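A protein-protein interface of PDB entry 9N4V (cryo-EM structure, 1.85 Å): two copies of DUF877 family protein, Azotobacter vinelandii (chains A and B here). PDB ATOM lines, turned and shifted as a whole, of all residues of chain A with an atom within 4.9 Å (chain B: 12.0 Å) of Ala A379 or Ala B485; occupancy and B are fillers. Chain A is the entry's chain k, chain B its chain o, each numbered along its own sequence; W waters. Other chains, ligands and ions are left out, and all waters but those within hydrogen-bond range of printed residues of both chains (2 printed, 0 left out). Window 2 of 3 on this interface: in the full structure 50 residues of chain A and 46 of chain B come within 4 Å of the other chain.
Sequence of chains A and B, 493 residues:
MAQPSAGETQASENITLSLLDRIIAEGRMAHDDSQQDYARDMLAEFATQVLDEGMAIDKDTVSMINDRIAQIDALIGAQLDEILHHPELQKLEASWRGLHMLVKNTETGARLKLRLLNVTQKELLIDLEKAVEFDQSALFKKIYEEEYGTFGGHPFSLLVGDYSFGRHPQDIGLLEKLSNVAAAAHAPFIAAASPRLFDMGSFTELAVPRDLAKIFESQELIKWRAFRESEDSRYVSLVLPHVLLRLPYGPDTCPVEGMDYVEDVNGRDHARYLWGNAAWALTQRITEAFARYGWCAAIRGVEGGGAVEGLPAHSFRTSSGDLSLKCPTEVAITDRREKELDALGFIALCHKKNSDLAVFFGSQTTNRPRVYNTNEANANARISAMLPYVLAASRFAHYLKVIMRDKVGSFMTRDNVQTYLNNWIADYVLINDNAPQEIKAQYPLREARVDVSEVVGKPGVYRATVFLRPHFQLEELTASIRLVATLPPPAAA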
ATOM      1  N   ASN A 375      26.843 -21.671  -7.518  1.00  0.00           N
ATOM      2  CA  ASN A 375      27.039 -20.233  -7.363  1.00  0.00           C
ATOM      3  C   ASN A 375      25.881 -19.590  -6.610  1.00  0.00           C
ATOM      4  O   ASN A 375      26.095 -18.713  -5.768  1.00  0.00           O
ATOM      5  CB  ASN A 375      27.216 -19.578  -8.733  1.00  0.00           C
ATOM      6  CG  ASN A 375      28.460 -20.055  -9.448  1.00  0.00           C
ATOM      7  OD1 ASN A 375      29.443 -20.434  -8.819  1.00  0.00           O
ATOM      8  ND2 ASN A 375      28.421 -20.040 -10.771  1.00  0.00           N
ATOM      9  N   GLU A 376      24.650 -20.006  -6.906  1.00  0.00           N
ATOM     10  CA  GLU A 376      23.484 -19.416  -6.255  1.00  0.00           C
ATOM     11  C   GLU A 376      23.519 -19.632  -4.747  1.00  0.00           C
ATOM     12  O   GLU A 376      23.287 -18.699  -3.971  1.00  0.00           O
ATOM     13  CB  GLU A 376      22.196 -19.989  -6.849  1.00  0.00           C
ATOM     14  CG  GLU A 376      21.933 -19.655  -8.319  1.00  0.00           C
ATOM     15  CD  GLU A 376      22.950 -20.242  -9.282  1.00  0.00           C
ATOM     16  OE1 GLU A 376      23.372 -19.519 -10.208  1.00  0.00           O
ATOM     17  OE2 GLU A 376      23.334 -21.420  -9.118  1.00  0.00           O
ATOM     18  N   ALA A 377      23.813 -20.860  -4.313  1.00  0.00           N
ATOM     19  CA  ALA A 377      23.853 -21.138  -2.883  1.00  0.00           C
ATOM     20  C   ALA A 377      24.973 -20.367  -2.203  1.00  0.00           C
ATOM     21  O   ALA A 377      24.788 -19.846  -1.099  1.00  0.00           O
ATOM     22  CB  ALA A 377      24.007 -22.635  -2.633  1.00  0.00           C
ATOM     23  N   ASN A 378      26.145 -20.297  -2.839  1.00  0.00           N
ATOM     24  CA  ASN A 378      27.255 -19.545  -2.262  1.00  0.00           C
ATOM     25  C   ASN A 378      26.896 -18.073  -2.117  1.00  0.00           C
ATOM     26  O   ASN A 378      27.094 -17.475  -1.055  1.00  0.00           O
ATOM     27  CB  ASN A 378      28.510 -19.718  -3.119  1.00  0.00           C
ATOM     28  CG  ASN A 378      29.199 -21.045  -2.878  1.00  0.00           C
ATOM     29  OD1 ASN A 378      29.253 -21.528  -1.754  1.00  0.00           O
ATOM     30  ND2 ASN A 378      29.734 -21.635  -3.934  1.00  0.00           N
ATOM     31  N   ALA A 379      26.339 -17.479  -3.174  1.00  0.00           N
ATOM     32  CA  ALA A 379      25.934 -16.080  -3.107  1.00  0.00           C
ATOM     33  C   ALA A 379      24.914 -15.857  -1.999  1.00  0.00           C
ATOM     34  O   ALA A 379      25.043 -14.918  -1.207  1.00  0.00           O
ATOM     35  CB  ALA A 379      25.375 -15.632  -4.456  1.00  0.00           C
ATOM     36  N   ASN A 380      23.905 -16.727  -1.909  1.00  0.00           N
ATOM     37  CA  ASN A 380      22.870 -16.547  -0.896  1.00  0.00           C
ATOM     38  C   ASN A 380      23.440 -16.689   0.508  1.00  0.00           C
ATOM     39  O   ASN A 380      23.080 -15.926   1.407  1.00  0.00           O
ATOM     40  CB  ASN A 380      21.727 -17.535  -1.125  1.00  0.00           C
ATOM     41  CG  ASN A 380      21.036 -17.322  -2.457  1.00  0.00           C
ATOM     42  OD1 ASN A 380      21.182 -16.278  -3.076  1.00  0.00           O
ATOM     43  ND2 ASN A 380      20.288 -18.316  -2.903  1.00  0.00           N
ATOM     44  N   ALA A 381      24.339 -17.655   0.714  1.00  0.00           N
ATOM     45  CA  ALA A 381      24.965 -17.808   2.021  1.00  0.00           C
ATOM     46  C   ALA A 381      25.776 -16.573   2.383  1.00  0.00           C
ATOM     47  O   ALA A 381      25.753 -16.121   3.532  1.00  0.00           O
ATOM     48  CB  ALA A 381      25.852 -19.052   2.043  1.00  0.00           C
ATOM     49  N   ARG A 382      26.497 -16.011   1.412  1.00  0.00           N
ATOM     50  CA  ARG A 382      27.358 -14.865   1.696  1.00  0.00           C
ATOM     51  C   ARG A 382      26.543 -13.644   2.108  1.00  0.00           C
ATOM     52  O   ARG A 382      26.853 -12.992   3.108  1.00  0.00           O
ATOM     53  CB  ARG A 382      28.232 -14.555   0.483  1.00  0.00           C
ATOM     54  CG  ARG A 382      29.355 -15.556   0.275  1.00  0.00           C
ATOM     55  CD  ARG A 382      29.964 -15.426  -1.106  1.00  0.00           C
ATOM     56  NE  ARG A 382      30.633 -14.144  -1.289  1.00  0.00           N
ATOM     57  CZ  ARG A 382      31.918 -13.933  -1.045  1.00  0.00           C
ATOM     58  NH1 ARG A 382      32.703 -14.897  -0.597  1.00  0.00           N
ATOM     59  NH2 ARG A 382      32.428 -12.726  -1.262  1.00  0.00           N
ATOM     60  N   ILE A 383      25.484 -13.327   1.360  1.00  0.00           N
ATOM     61  CA  ILE A 383      24.698 -12.142   1.681  1.00  0.00           C
ATOM     62  C   ILE A 383      23.855 -12.342   2.934  1.00  0.00           C
ATOM     63  O   ILE A 383      23.478 -11.361   3.582  1.00  0.00           O
ATOM     64  CB  ILE A 383      23.821 -11.732   0.486  1.00  0.00           C
ATOM     65  CG1 ILE A 383      22.818 -12.833   0.140  1.00  0.00           C
ATOM     66  CG2 ILE A 383      24.689 -11.408  -0.720  1.00  0.00           C
ATOM     67  CD1 ILE A 383      21.895 -12.464  -0.991  1.00  0.00           C
ATOM     68  N   ARG A 469      15.540  -9.822  -2.872  1.00  0.00           N
ATOM     69  CA  ARG A 469      16.793  -9.544  -3.561  1.00  0.00           C
ATOM     70  C   ARG A 469      17.196  -8.096  -3.320  1.00  0.00           C
ATOM     71  O   ARG A 469      16.600  -7.186  -3.913  1.00  0.00           O
ATOM     72  CB  ARG A 469      16.668  -9.820  -5.055  1.00  0.00           C
ATOM     73  CG  ARG A 469      17.970  -9.625  -5.806  1.00  0.00           C
ATOM     74  CD  ARG A 469      17.728  -9.564  -7.291  1.00  0.00           C
ATOM     75  NE  ARG A 469      18.820  -8.924  -8.010  1.00  0.00           N
ATOM     76  CZ  ARG A 469      18.844  -8.764  -9.326  1.00  0.00           C
ATOM     77  NH1 ARG A 469      17.851  -9.185 -10.089  1.00  0.00           N
ATOM     78  NH2 ARG A 469      19.890  -8.165  -9.888  1.00  0.00           N
ATOM     79  N   PHE A 472      22.961  -4.693  -4.073  1.00  0.00           N
ATOM     80  CA  PHE A 472      24.218  -5.160  -3.504  1.00  0.00           C
ATOM     81  C   PHE A 472      25.264  -4.055  -3.473  1.00  0.00           C
ATOM     82  O   PHE A 472      25.365  -3.245  -4.395  1.00  0.00           O
ATOM     83  CB  PHE A 472      24.738  -6.370  -4.275  1.00  0.00           C
ATOM     84  CG  PHE A 472      23.863  -7.575  -4.128  1.00  0.00           C
ATOM     85  CD1 PHE A 472      23.561  -8.071  -2.874  1.00  0.00           C
ATOM     86  CD2 PHE A 472      23.309  -8.184  -5.234  1.00  0.00           C
ATOM     87  CE1 PHE A 472      22.736  -9.171  -2.728  1.00  0.00           C
ATOM     88  CE2 PHE A 472      22.490  -9.284  -5.094  1.00  0.00           C
ATOM     89  CZ  PHE A 472      22.201  -9.773  -3.839  1.00  0.00           C
ATOM     90  N   ILE B 481      11.672 -16.188   5.254  1.00  0.00           N
ATOM     91  CA  ILE B 481      12.266 -15.066   4.538  1.00  0.00           C
ATOM     92  C   ILE B 481      13.661 -15.466   4.086  1.00  0.00           C
ATOM     93  O   ILE B 481      14.442 -16.015   4.870  1.00  0.00           O
ATOM     94  CB  ILE B 481      12.310 -13.804   5.412  1.00  0.00           C
ATOM     95  CG1 ILE B 481      10.892 -13.384   5.797  1.00  0.00           C
ATOM     96  CG2 ILE B 481      13.021 -12.684   4.679  1.00  0.00           C
ATOM     97  CD1 ILE B 481      10.857 -12.279   6.780  1.00  0.00           C
ATOM     98  N   ARG B 482      13.976 -15.201   2.821  1.00  0.00           N
ATOM     99  CA  ARG B 482      15.240 -15.633   2.239  1.00  0.00           C
ATOM    100  C   ARG B 482      15.818 -14.534   1.359  1.00  0.00           C
ATOM    101  O   ARG B 482      15.198 -14.139   0.369  1.00  0.00           O
ATOM    102  CB  ARG B 482      15.046 -16.923   1.438  1.00  0.00           C
ATOM    103  CG  ARG B 482      14.555 -18.070   2.292  1.00  0.00           C
ATOM    104  CD  ARG B 482      13.989 -19.200   1.484  1.00  0.00           C
ATOM    105  NE  ARG B 482      13.404 -20.203   2.363  1.00  0.00           N
ATOM    106  CZ  ARG B 482      13.322 -21.493   2.078  1.00  0.00           C
ATOM    107  NH1 ARG B 482      13.767 -21.976   0.931  1.00  0.00           N
ATOM    108  NH2 ARG B 482      12.777 -22.318   2.967  1.00  0.00           N
ATOM    109  N   LEU B 483      17.003 -14.046   1.723  1.00  0.00           N
ATOM    110  CA  LEU B 483      17.755 -13.145   0.860  1.00  0.00           C
ATOM    111  C   LEU B 483      18.374 -13.949  -0.274  1.00  0.00           C
ATOM    112  O   LEU B 483      18.989 -14.989  -0.035  1.00  0.00           O
ATOM    113  CB  LEU B 483      18.847 -12.423   1.648  1.00  0.00           C
ATOM    114  CG  LEU B 483      18.403 -11.402   2.691  1.00  0.00           C
ATOM    115  CD1 LEU B 483      19.466 -11.240   3.756  1.00  0.00           C
ATOM    116  CD2 LEU B 483      18.092 -10.075   2.018  1.00  0.00           C
ATOM    117  N   VAL B 484      18.213 -13.476  -1.504  1.00  0.00           N
ATOM    118  CA  VAL B 484      18.731 -14.182  -2.669  1.00  0.00           C
ATOM    119  C   VAL B 484      19.410 -13.191  -3.605  1.00  0.00           C
ATOM    120  O   VAL B 484      18.973 -12.044  -3.737  1.00  0.00           O
ATOM    121  CB  VAL B 484      17.621 -14.961  -3.408  1.00  0.00           C
ATOM    122  CG1 VAL B 484      17.065 -16.076  -2.524  1.00  0.00           C
ATOM    123  CG2 VAL B 484      16.515 -14.023  -3.872  1.00  0.00           C
ATOM    124  N   ALA B 485      20.483 -13.636  -4.257  1.00  0.00           N
ATOM    125  CA  ALA B 485      21.071 -12.843  -5.329  1.00  0.00           C
ATOM    126  C   ALA B 485      20.237 -12.910  -6.599  1.00  0.00           C
ATOM    127  O   ALA B 485      20.214 -11.947  -7.369  1.00  0.00           O
ATOM    128  CB  ALA B 485      22.501 -13.298  -5.614  1.00  0.00           C
ATOM    129  N   THR B 486      19.557 -14.029  -6.834  1.00  0.00           N
ATOM    130  CA  THR B 486      18.631 -14.178  -7.947  1.00  0.00           C
ATOM    131  C   THR B 486      17.369 -14.874  -7.454  1.00  0.00           C
ATOM    132  O   THR B 486      17.442 -15.778  -6.619  1.00  0.00           O
ATOM    133  CB  THR B 486      19.250 -14.987  -9.100  1.00  0.00           C
ATOM    134  OG1 THR B 486      19.734 -16.239  -8.601  1.00  0.00           O
ATOM    135  CG2 THR B 486      20.405 -14.231  -9.734  1.00  0.00           C
ATOM    136  N   LEU B 487      16.223 -14.452  -7.967  1.00  0.00           N
ATOM    137  CA  LEU B 487      14.957 -15.086  -7.604  1.00  0.00           C
ATOM    138  C   LEU B 487      14.900 -16.495  -8.180  1.00  0.00           C
ATOM    139  O   LEU B 487      15.026 -16.659  -9.397  1.00  0.00           O
ATOM    140  CB  LEU B 487      13.773 -14.278  -8.127  1.00  0.00           C
ATOM    141  CG  LEU B 487      13.355 -12.963  -7.476  1.00  0.00           C
ATOM    142  CD1 LEU B 487      11.963 -12.591  -7.959  1.00  0.00           C
ATOM    143  CD2 LEU B 487      13.386 -13.062  -5.971  1.00  0.00           C
ATOM    144  N   PRO B 488      14.715 -17.526  -7.366  1.00  0.00           N
ATOM    145  CA  PRO B 488      14.495 -18.867  -7.911  1.00  0.00           C
ATOM    146  C   PRO B 488      13.093 -18.987  -8.480  1.00  0.00           C
ATOM    147  O   PRO B 488      12.199 -18.215  -8.107  1.00  0.00           O
ATOM    148  CB  PRO B 488      14.688 -19.779  -6.692  1.00  0.00           C
ATOM    149  CG  PRO B 488      14.383 -18.925  -5.534  1.00  0.00           C
ATOM    150  CD  PRO B 488      14.767 -17.523  -5.895  1.00  0.00           C
ATOM    151  N   PRO B 489      12.863 -19.930  -9.399  1.00  0.00           N
ATOM    152  CA  PRO B 489      11.506 -20.137  -9.900  1.00  0.00           C
ATOM    153  C   PRO B 489      10.602 -20.668  -8.804  1.00  0.00           C
ATOM    154  O   PRO B 489      11.068 -21.334  -7.865  1.00  0.00           O
ATOM    155  CB  PRO B 489      11.699 -21.174 -11.023  1.00  0.00           C
ATOM    156  CG  PRO B 489      12.978 -21.857 -10.690  1.00  0.00           C
ATOM    157  CD  PRO B 489      13.841 -20.815 -10.051  1.00  0.00           C
HETATM  158  O   HOH W   1      21.341 -16.494  -5.614  1.00  0.00           O
HETATM  159  O   HOH W   2      18.872 -17.886  -5.648  1.00  0.00           O
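N of Ala B485 is in hydrogen-bond range of OD1 of Asn A380 (3.0 Å). O of Ala B485 is in hydrogen-bond range of NE of Arg A469, 3.4 Å away.
O of Glu A376 sits close to ND2 of Asn A380, 3.2 Å away.
Ala A379 touches Ala B485 (CB to CB, 3.9 Å). Leu B483 touches Asn A380. OD1 of Asn A380 touches CA of Val B484 (3.3 Å). Ile A383 touches Leu B483. Ile A383 touches Val B484 (CD1 to C, 3.7 Å). Ala B485 touches Ile A383. O of Val B484 touches CA of Arg A469, at 3.3 Å. Val B484 touches Phe A472 (O to CZ, 3.9 Å). CA of Ala B485 touches CZ of Phe A472, at 3.6 Å.
Of chain B, only Ala B485 (3.9 Å) comes within 4 Å of Ala A379. Ala B485 touches just these residues of chain A: Ala A379 (3.9 Å), Asn A380 (3.0 Å), Ile A383 (3.7 Å), Arg A469 (3.4 Å) and Phe A472 (3.6 Å). No residue of chain B comes within 4 Å of Glu A376. No residue of chain B comes within 4 Å of Asn A378. No residue of chain B comes within 4 Å of Ala A381. No residue of chain B comes within 4 Å of Arg A382. Of chain B, only Leu B483, Val B484 and Ala B485 come within 4 Å of Ile A383. Arg A469 touches just these residues of chain B: Val B484 and Ala B485. Of the printed residues of chain B, Phe A472 touches Val B484 (3.9 Å) and Ala B485 (3.6 Å). Of the printed residues of chain A, Val B484 touches Asn A380 (3.3 Å), Ile A383 (3.7 Å), Arg A469 (3.3 Å) and Phe A472 (3.9 Å). Printed residues of chain A within 4 Å of Leu B483: Asn A380 and Ile A383. Pro B488 touches none of the printed residues of chain A. The nearest printed residue of chain A that does not touch Leu B483 is Arg A469 (5.5 Å).
Of the 11 printed residues of chain A, 5 touch a printed residue of chain B. Printed residues of chain A that touch a printed residue of chain B: Ala A379, Asn A380, Ile A383, Arg A469 and Phe A472. Hydrophobic or aromatic side chains of chain A that line the printed part of chain B: Ala A379, Ile A383 and Phe A472. Printed residues of chain B that touch a printed residue of chain A: Leu B483, Val B484 and Ala B485. Among the printed residues, 11 pairs touch across the chains.
No position is printed for both chains. Of the 11 pairs that touch across the chains among the printed residues, none has its exchanged pair printed and touching as well.
Water W1 lies within hydrogen-bond range of the side-chain amide oxygen (OD1) of Asn A380 (2.6 Å), the backbone NH (N) of Ala B485 (3.3 Å), the backbone NH (N) of Thr B486 (3.3 Å) and the backbone carbonyl oxygen (O) of Glu A376 (3.4 Å). Water W2 lies within hydrogen-bond range of O of Thr B486 (2.7 Å) and ND2 of Asn A380 (3.1 Å).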
